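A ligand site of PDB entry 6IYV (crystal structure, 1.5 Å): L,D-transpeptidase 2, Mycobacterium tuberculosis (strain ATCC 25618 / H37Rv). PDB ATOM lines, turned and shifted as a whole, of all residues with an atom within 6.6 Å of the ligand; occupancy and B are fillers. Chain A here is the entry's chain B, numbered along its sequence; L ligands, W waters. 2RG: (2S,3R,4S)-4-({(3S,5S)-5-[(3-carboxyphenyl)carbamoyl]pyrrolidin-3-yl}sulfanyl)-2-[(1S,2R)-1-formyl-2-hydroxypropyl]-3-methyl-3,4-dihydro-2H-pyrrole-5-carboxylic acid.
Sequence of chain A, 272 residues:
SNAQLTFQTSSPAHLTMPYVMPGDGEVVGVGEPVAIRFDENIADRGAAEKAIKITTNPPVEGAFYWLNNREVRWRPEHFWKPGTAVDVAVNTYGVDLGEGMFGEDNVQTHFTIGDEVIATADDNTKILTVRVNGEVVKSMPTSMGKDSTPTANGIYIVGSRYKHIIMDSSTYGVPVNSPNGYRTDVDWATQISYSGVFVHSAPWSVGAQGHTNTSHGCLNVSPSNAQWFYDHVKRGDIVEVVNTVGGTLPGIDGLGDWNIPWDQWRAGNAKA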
ATOM      1  N   THR A 149     -13.201   7.509  33.011  1.00  0.00           N
ATOM      2  CA  THR A 149     -11.990   7.046  32.331  1.00  0.00           C
ATOM      3  C   THR A 149     -10.903   6.901  33.386  1.00  0.00           C
ATOM      4  O   THR A 149      -9.896   7.614  33.373  1.00  0.00           O
ATOM      5  CB  THR A 149     -11.561   8.002  31.224  1.00  0.00           C
ATOM      6  OG1 THR A 149     -11.260   9.294  31.784  1.00  0.00           O
ATOM      7  CG2 THR A 149     -12.652   8.160  30.164  1.00  0.00           C
ATOM      8  N   PRO A 150     -11.084   5.983  34.325  1.00  0.00           N
ATOM      9  CA  PRO A 150     -10.209   5.952  35.509  1.00  0.00           C
ATOM     10  C   PRO A 150      -8.854   5.341  35.202  1.00  0.00           C
ATOM     11  O   PRO A 150      -8.659   4.639  34.203  1.00  0.00           O
ATOM     12  CB  PRO A 150     -10.996   5.088  36.490  1.00  0.00           C
ATOM     13  CG  PRO A 150     -11.781   4.165  35.614  1.00  0.00           C
ATOM     14  CD  PRO A 150     -12.155   4.976  34.400  1.00  0.00           C
ATOM     15  N   ILE A 166       3.369  14.374  21.697  1.00  0.00           N
ATOM     16  CA  ILE A 166       1.984  14.755  21.455  1.00  0.00           C
ATOM     17  C   ILE A 166       1.072  13.590  21.810  1.00  0.00           C
ATOM     18  O   ILE A 166       1.261  12.475  21.315  1.00  0.00           O
ATOM     19  CB  ILE A 166       1.771  15.154  19.985  1.00  0.00           C
ATOM     20  CG1 ILE A 166       2.717  16.271  19.585  1.00  0.00           C
ATOM     21  CG2 ILE A 166       0.313  15.577  19.773  1.00  0.00           C
ATOM     22  CD1 ILE A 166       2.367  17.583  20.204  1.00  0.00           C
ATOM     23  N   MET A 167       0.075  13.849  22.640  1.00  0.00           N
ATOM     24  CA  MET A 167      -0.981  12.884  22.944  1.00  0.00           C
ATOM     25  C   MET A 167      -2.247  13.273  22.189  1.00  0.00           C
ATOM     26  O   MET A 167      -2.710  14.421  22.279  1.00  0.00           O
ATOM     27  CB  MET A 167      -1.194  12.778  24.449  1.00  0.00           C
ATOM     28  CG  MET A 167       0.074  12.249  25.105  1.00  0.00           C
ATOM     29  SD  MET A 167       0.122  12.195  26.890  1.00  0.00           S
ATOM     30  CE  MET A 167       1.834  11.674  27.101  1.00  0.00           C
ATOM     31  N   ASP A 168      -2.760  12.345  21.378  1.00  0.00           N
ATOM     32  CA  ASP A 168      -3.780  12.610  20.369  1.00  0.00           C
ATOM     33  C   ASP A 168      -4.838  11.515  20.380  1.00  0.00           C
ATOM     34  O   ASP A 168      -4.520  10.343  20.179  1.00  0.00           O
ATOM     35  CB  ASP A 168      -3.073  12.734  19.009  1.00  0.00           C
ATOM     36  CG  ASP A 168      -4.007  13.077  17.860  1.00  0.00           C
ATOM     37  OD1 ASP A 168      -5.136  12.573  17.804  1.00  0.00           O
ATOM     38  OD2 ASP A 168      -3.573  13.851  16.966  1.00  0.00           O
ATOM     39  N   SER A 169      -6.100  11.893  20.635  1.00  0.00           N
ATOM     40  CA  SER A 169      -7.172  10.894  20.746  1.00  0.00           C
ATOM     41  C   SER A 169      -7.425  10.165  19.435  1.00  0.00           C
ATOM     42  O   SER A 169      -7.978   9.062  19.446  1.00  0.00           O
ATOM     43  CB  SER A 169      -8.470  11.557  21.232  1.00  0.00           C
ATOM     44  OG  SER A 169      -8.926  12.516  20.297  1.00  0.00           O
ATOM     45  N   THR A 171      -5.473   8.639  17.647  1.00  0.00           N
ATOM     46  CA  THR A 171      -4.698   7.415  17.503  1.00  0.00           C
ATOM     47  C   THR A 171      -5.449   6.188  17.985  1.00  0.00           C
ATOM     48  O   THR A 171      -5.062   5.069  17.622  1.00  0.00           O
ATOM     49  CB  THR A 171      -3.352   7.524  18.237  1.00  0.00           C
ATOM     50  OG1 THR A 171      -3.578   7.602  19.650  1.00  0.00           O
ATOM     51  CG2 THR A 171      -2.579   8.743  17.773  1.00  0.00           C
ATOM     52  N   TYR A 172      -6.506   6.356  18.772  1.00  0.00           N
ATOM     53  CA  TYR A 172      -7.361   5.233  19.136  1.00  0.00           C
ATOM     54  C   TYR A 172      -8.771   5.357  18.576  1.00  0.00           C
ATOM     55  O   TYR A 172      -9.655   4.580  18.969  1.00  0.00           O
ATOM     56  CB  TYR A 172      -7.388   5.022  20.648  1.00  0.00           C
ATOM     57  CG  TYR A 172      -7.911   6.162  21.495  1.00  0.00           C
ATOM     58  CD1 TYR A 172      -9.278   6.379  21.662  1.00  0.00           C
ATOM     59  CD2 TYR A 172      -7.039   6.992  22.196  1.00  0.00           C
ATOM     60  CE1 TYR A 172      -9.752   7.394  22.462  1.00  0.00           C
ATOM     61  CE2 TYR A 172      -7.504   8.012  22.998  1.00  0.00           C
ATOM     62  CZ  TYR A 172      -8.865   8.208  23.134  1.00  0.00           C
ATOM     63  OH  TYR A 172      -9.339   9.219  23.943  1.00  0.00           O
ATOM     64  N   GLY A 173      -9.007   6.282  17.648  1.00  0.00           N
ATOM     65  CA  GLY A 173     -10.278   6.355  16.945  1.00  0.00           C
ATOM     66  C   GLY A 173     -11.242   7.463  17.310  1.00  0.00           C
ATOM     67  O   GLY A 173     -12.372   7.456  16.801  1.00  0.00           O
ATOM     68  N   VAL A 174     -10.852   8.415  18.153  1.00  0.00           N
ATOM     69  CA  VAL A 174     -11.722   9.527  18.498  1.00  0.00           C
ATOM     70  C   VAL A 174     -11.172  10.775  17.814  1.00  0.00           C
ATOM     71  O   VAL A 174     -10.066  11.233  18.158  1.00  0.00           O
ATOM     72  CB  VAL A 174     -11.846   9.717  20.019  1.00  0.00           C
ATOM     73  CG1 VAL A 174     -12.643  10.979  20.325  1.00  0.00           C
ATOM     74  CG2 VAL A 174     -12.503   8.503  20.651  1.00  0.00           C
ATOM     75  N   ASN A 180     -15.089  15.043  22.661  1.00  0.00           N
ATOM     76  CA  ASN A 180     -14.216  14.346  23.600  1.00  0.00           C
ATOM     77  C   ASN A 180     -12.842  14.062  23.015  1.00  0.00           C
ATOM     78  O   ASN A 180     -12.050  13.343  23.624  1.00  0.00           O
ATOM     79  CB  ASN A 180     -14.879  13.048  24.050  1.00  0.00           C
ATOM     80  CG  ASN A 180     -15.224  12.131  22.893  1.00  0.00           C
ATOM     81  OD1 ASN A 180     -15.667  12.590  21.835  1.00  0.00           O
ATOM     82  ND2 ASN A 180     -15.027  10.832  23.084  1.00  0.00           N
ATOM     83  N   TYR A 182      -8.958  15.237  21.596  1.00  0.00           N
ATOM     84  CA  TYR A 182      -7.904  16.129  22.074  1.00  0.00           C
ATOM     85  C   TYR A 182      -6.644  15.907  21.263  1.00  0.00           C
ATOM     86  O   TYR A 182      -6.402  14.815  20.735  1.00  0.00           O
ATOM     87  CB  TYR A 182      -7.631  15.924  23.558  1.00  0.00           C
ATOM     88  CG  TYR A 182      -7.185  14.535  23.941  1.00  0.00           C
ATOM     89  CD1 TYR A 182      -5.859  14.154  23.807  1.00  0.00           C
ATOM     90  CD2 TYR A 182      -8.084  13.593  24.455  1.00  0.00           C
ATOM     91  CE1 TYR A 182      -5.429  12.888  24.147  1.00  0.00           C
ATOM     92  CE2 TYR A 182      -7.663  12.318  24.803  1.00  0.00           C
ATOM     93  CZ  TYR A 182      -6.338  11.970  24.651  1.00  0.00           C
ATOM     94  OH  TYR A 182      -5.872  10.701  24.990  1.00  0.00           O
ATOM     95  N   SER A 193       2.744   2.241  31.058  1.00  0.00           N
ATOM     96  CA  SER A 193       2.082   1.060  30.492  1.00  0.00           C
ATOM     97  C   SER A 193       2.122   1.133  28.971  1.00  0.00           C
ATOM     98  O   SER A 193       2.230   2.227  28.400  1.00  0.00           O
ATOM     99  CB  SER A 193       0.612   0.943  30.922  1.00  0.00           C
ATOM    100  OG  SER A 193      -0.238   1.790  30.152  1.00  0.00           O
ATOM    101  N   SER A 195      -0.501   0.283  27.331  1.00  0.00           N
ATOM    102  CA  SER A 195      -1.821   0.802  27.011  1.00  0.00           C
ATOM    103  C   SER A 195      -1.816   2.311  26.875  1.00  0.00           C
ATOM    104  O   SER A 195      -2.794   2.884  26.395  1.00  0.00           O
ATOM    105  CB  SER A 195      -2.838   0.362  28.078  1.00  0.00           C
ATOM    106  OG  SER A 195      -2.529   0.872  29.365  1.00  0.00           O
ATOM    107  N   GLY A 196      -0.730   2.964  27.286  1.00  0.00           N
ATOM    108  CA  GLY A 196      -0.541   4.374  27.062  1.00  0.00           C
ATOM    109  C   GLY A 196      -0.577   5.242  28.292  1.00  0.00           C
ATOM    110  O   GLY A 196      -0.728   6.464  28.165  1.00  0.00           O
ATOM    111  N   VAL A 197      -0.464   4.668  29.493  1.00  0.00           N
ATOM    112  CA  VAL A 197      -0.462   5.463  30.712  1.00  0.00           C
ATOM    113  C   VAL A 197       0.920   6.088  30.892  1.00  0.00           C
ATOM    114  O   VAL A 197       1.946   5.411  30.762  1.00  0.00           O
ATOM    115  CB  VAL A 197      -0.838   4.600  31.929  1.00  0.00           C
ATOM    116  CG1 VAL A 197      -0.789   5.446  33.184  1.00  0.00           C
ATOM    117  CG2 VAL A 197      -2.235   4.029  31.752  1.00  0.00           C
ATOM    118  N   PHE A 198       0.927   7.383  31.197  1.00  0.00           N
ATOM    119  CA  PHE A 198       2.129   8.160  31.436  1.00  0.00           C
ATOM    120  C   PHE A 198       1.986   8.962  32.723  1.00  0.00           C
ATOM    121  O   PHE A 198       0.877   9.396  33.082  1.00  0.00           O
ATOM    122  CB  PHE A 198       2.420   9.210  30.328  1.00  0.00           C
ATOM    123  CG  PHE A 198       2.856   8.651  29.033  1.00  0.00           C
ATOM    124  CD1 PHE A 198       1.943   8.108  28.145  1.00  0.00           C
ATOM    125  CD2 PHE A 198       4.186   8.751  28.649  1.00  0.00           C
ATOM    126  CE1 PHE A 198       2.366   7.621  26.896  1.00  0.00           C
ATOM    127  CE2 PHE A 198       4.617   8.255  27.429  1.00  0.00           C
ATOM    128  CZ  PHE A 198       3.700   7.692  26.553  1.00  0.00           C
ATOM    129  N   HIS A 200       3.214  12.644  33.586  1.00  0.00           N
ATOM    130  CA  HIS A 200       3.674  13.724  32.714  1.00  0.00           C
ATOM    131  C   HIS A 200       3.280  15.080  33.286  1.00  0.00           C
ATOM    132  O   HIS A 200       2.456  15.185  34.189  1.00  0.00           O
ATOM    133  CB  HIS A 200       3.115  13.572  31.304  1.00  0.00           C
ATOM    134  CG  HIS A 200       1.635  13.728  31.210  1.00  0.00           C
ATOM    135  ND1 HIS A 200       1.012  14.955  31.192  1.00  0.00           N
ATOM    136  CD2 HIS A 200       0.649  12.804  31.137  1.00  0.00           C
ATOM    137  CE1 HIS A 200      -0.292  14.776  31.099  1.00  0.00           C
ATOM    138  NE2 HIS A 200      -0.538  13.487  31.070  1.00  0.00           N
ATOM    139  N   SER A 215      -8.168  13.548  34.415  1.00  0.00           N
ATOM    140  CA  SER A 215      -7.461  13.105  33.222  1.00  0.00           C
ATOM    141  C   SER A 215      -8.207  11.985  32.497  1.00  0.00           C
ATOM    142  O   SER A 215      -9.272  11.509  32.929  1.00  0.00           O
ATOM    143  CB  SER A 215      -6.045  12.654  33.575  1.00  0.00           C
ATOM    144  OG  SER A 215      -6.050  11.307  34.040  1.00  0.00           O
ATOM    145  N   HIS A 216      -7.627  11.534  31.376  1.00  0.00           N
ATOM    146  CA  HIS A 216      -8.140  10.372  30.666  1.00  0.00           C
ATOM    147  C   HIS A 216      -7.552   9.067  31.188  1.00  0.00           C
ATOM    148  O   HIS A 216      -7.838   8.000  30.623  1.00  0.00           O
ATOM    149  CB  HIS A 216      -7.859  10.480  29.163  1.00  0.00           C
ATOM    150  CG  HIS A 216      -8.535  11.653  28.512  1.00  0.00           C
ATOM    151  ND1 HIS A 216      -7.934  12.879  28.381  1.00  0.00           N
ATOM    152  CD2 HIS A 216      -9.761  11.774  27.953  1.00  0.00           C
ATOM    153  CE1 HIS A 216      -8.756  13.708  27.768  1.00  0.00           C
ATOM    154  NE2 HIS A 216      -9.872  13.068  27.506  1.00  0.00           N
ATOM    155  N   GLY A 217      -6.749   9.122  32.256  1.00  0.00           N
ATOM    156  CA  GLY A 217      -6.120   7.928  32.809  1.00  0.00           C
ATOM    157  C   GLY A 217      -4.649   8.157  33.147  1.00  0.00           C
ATOM    158  O   GLY A 217      -4.102   7.495  34.046  1.00  0.00           O
ATOM    159  N   CYS A 218      -4.019   9.101  32.466  1.00  0.00           N
ATOM    160  CA  CYS A 218      -2.640   9.467  32.768  1.00  0.00           C
ATOM    161  C   CYS A 218      -2.534  10.112  34.150  1.00  0.00           C
ATOM    162  O   CYS A 218      -3.489  10.650  34.702  1.00  0.00           O
ATOM    163  CB  CYS A 218      -2.077  10.407  31.710  1.00  0.00           C
ATOM    164  SG  CYS A 218      -1.676   9.522  30.176  1.00  0.00           S
ATOM    165  N   LEU A 219      -1.323  10.076  34.695  1.00  0.00           N
ATOM    166  CA  LEU A 219      -1.039  10.675  36.001  1.00  0.00           C
ATOM    167  C   LEU A 219      -0.496  12.088  35.769  1.00  0.00           C
ATOM    168  O   LEU A 219       0.678  12.264  35.452  1.00  0.00           O
ATOM    169  CB  LEU A 219      -0.059   9.827  36.805  1.00  0.00           C
ATOM    170  CG  LEU A 219      -0.688   8.645  37.541  1.00  0.00           C
ATOM    171  CD1 LEU A 219      -1.263   7.678  36.546  1.00  0.00           C
ATOM    172  CD2 LEU A 219       0.344   7.942  38.402  1.00  0.00           C
ATOM    173  N   ASN A 220      -1.375  13.088  35.908  1.00  0.00           N
ATOM    174  CA  ASN A 220      -0.972  14.483  35.777  1.00  0.00           C
ATOM    175  C   ASN A 220      -0.217  14.913  37.031  1.00  0.00           C
ATOM    176  O   ASN A 220      -0.709  14.706  38.144  1.00  0.00           O
ATOM    177  CB  ASN A 220      -2.188  15.386  35.659  1.00  0.00           C
ATOM    178  CG  ASN A 220      -2.939  15.276  34.344  1.00  0.00           C
ATOM    179  OD1 ASN A 220      -2.684  14.435  33.480  1.00  0.00           O
ATOM    180  ND2 ASN A 220      -3.934  16.154  34.216  1.00  0.00           N
HETATM  181  C   2RG L   1     -10.317   3.788  23.691  1.00  0.00           C
HETATM  182  N   2RG L   1      -9.031   2.642  25.462  1.00  0.00           N
HETATM  183  O   2RG L   1      -9.855   3.071  22.854  1.00  0.00           O
HETATM  184  CA  2RG L   1      -9.630   3.925  25.029  1.00  0.00           C
HETATM  185  CB  2RG L   1      -8.511   4.977  24.998  1.00  0.00           C
HETATM  186  CD  2RG L   1      -7.791   2.981  26.159  1.00  0.00           C
HETATM  187  CG  2RG L   1      -7.740   4.493  26.212  1.00  0.00           C
HETATM  188  CAA 2RG L   1      -3.211   9.308  29.260  1.00  0.00           C
HETATM  189  CAB 2RG L   1      -2.918   8.597  27.917  1.00  0.00           C
HETATM  190  OAC 2RG L   1      -4.245   9.852  29.505  1.00  0.00           O
HETATM  191  CAD 2RG L   1      -4.048   7.783  27.308  1.00  0.00           C
HETATM  192  CAE 2RG L   1      -2.359   9.618  26.896  1.00  0.00           C
HETATM  193  CAF 2RG L   1      -1.941   8.869  25.635  1.00  0.00           C
HETATM  194  OAG 2RG L   1      -3.296  10.606  26.631  1.00  0.00           O
HETATM  195  CAH 2RG L   1      -4.529   6.538  28.126  1.00  0.00           C
HETATM  196  CAI 2RG L   1      -5.936   6.392  27.584  1.00  0.00           C
HETATM  197  NAJ 2RG L   1      -5.286   8.495  27.057  1.00  0.00           N
HETATM  198  SAK 2RG L   1      -6.015   5.139  26.250  1.00  0.00           S
HETATM  199  CAL 2RG L   1      -6.216   7.743  27.064  1.00  0.00           C
HETATM  200  CAM 2RG L   1      -7.617   8.167  26.654  1.00  0.00           C
HETATM  201  CAS 2RG L   1      -4.540   6.700  29.613  1.00  0.00           C
HETATM  202  OAT 2RG L   1      -7.789   9.258  26.025  1.00  0.00           O
HETATM  203  OAU 2RG L   1      -8.608   7.446  26.951  1.00  0.00           O
HETATM  204  NAX 2RG L   1     -11.545   4.553  23.531  1.00  0.00           N
HETATM  205  CAY 2RG L   1     -12.397   4.589  22.338  1.00  0.00           C
HETATM  206  CAZ 2RG L   1     -12.142   3.754  21.268  1.00  0.00           C
HETATM  207  CBA 2RG L   1     -12.965   3.810  20.152  1.00  0.00           C
HETATM  208  CBB 2RG L   1     -14.029   4.689  20.122  1.00  0.00           C
HETATM  209  CBC 2RG L   1     -14.293   5.519  21.190  1.00  0.00           C
HETATM  210  CBD 2RG L   1     -13.462   5.467  22.309  1.00  0.00           C
HETATM  211  CBE 2RG L   1     -12.695   2.884  18.973  1.00  0.00           C
HETATM  212  OBF 2RG L   1     -11.736   2.072  19.021  1.00  0.00           O
HETATM  213  OBG 2RG L   1     -13.431   2.925  17.949  1.00  0.00           O
HETATM  214  O   HOH W   1      -4.258   9.148  23.144  1.00  0.00           O
HETATM  215  O   HOH W   2     -11.251   2.619  27.949  1.00  0.00           O
HETATM  216  O   HOH W   3     -12.566   6.031  25.578  1.00  0.00           O
HETATM  217  O   HOH W   4     -11.398   7.921  26.765  1.00  0.00           O
HETATM  218  O   HOH W   5      -9.267   0.132  24.855  1.00  0.00           O
HETATM  219  O   HOH W   6      -2.853  12.837  28.390  1.00  0.00           O
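OAT of the ligand sits at hydrogen-bond distance from OH of Tyr 172, at 2.6 Å.
An oxygen (OAC) of the ligand sits at hydrogen-bond distance from the backbone NH (N) of Cys 218 (3.1 Å).
The side-chain hydroxyl (OH) of Tyr 182 lies within hydrogen-bond range of an oxygen (OAT) of the ligand (2.6 Å).
SD of Met 167 sits close to OAG of the ligand (3.8 Å).
SG of Cys 218 is covalently linked to CAA of the ligand, at 1.8 Å.
N of Gly 217 is in hydrogen-bond range of OG of Ser 215.
The side-chain hydroxyl (OG) of Ser 215 is in hydrogen-bond range of the backbone carbonyl oxygen (O) of Cys 218.
N of Ser 169 is in hydrogen-bond range of O of Tyr 182 (2.9 Å).
The backbone NH (N) of Phe 198 lies within hydrogen-bond range of the side-chain sulfur (SG) of Cys 218 (3.5 Å).
The side-chain hydroxyl of Ser 193 sits at hydrogen-bond distance from the side-chain hydroxyl of Ser 195.
OG of Ser 169 is in hydrogen-bond range of O of Val 174.
The side-chain hydroxyl of Ser 193 is in hydrogen-bond range of the backbone NH of Gly 196 (3.1 Å).
Residues that only touch the ligand: Val 174, Ser 195, Gly 196, His 216 and Gly 217.
Hydrophobic or aromatic side chains within 4 Å of the ligand: Met 167, Tyr 172, Val 174, Tyr 182 and His 216.
Within 4 Å of the ligand: Met 167, Tyr 172, Val 174, Tyr 182, Ser 195, Gly 196, His 216, Gly 217 and Cys 218.
Water W6 bridges an oxygen (OAG) of the ligand (2.9 Å) and the side-chain sulfur of Met 167 (3.4 Å).
Water W1 lies within hydrogen-bond range of OH of Tyr 182 and O of Asp 168.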
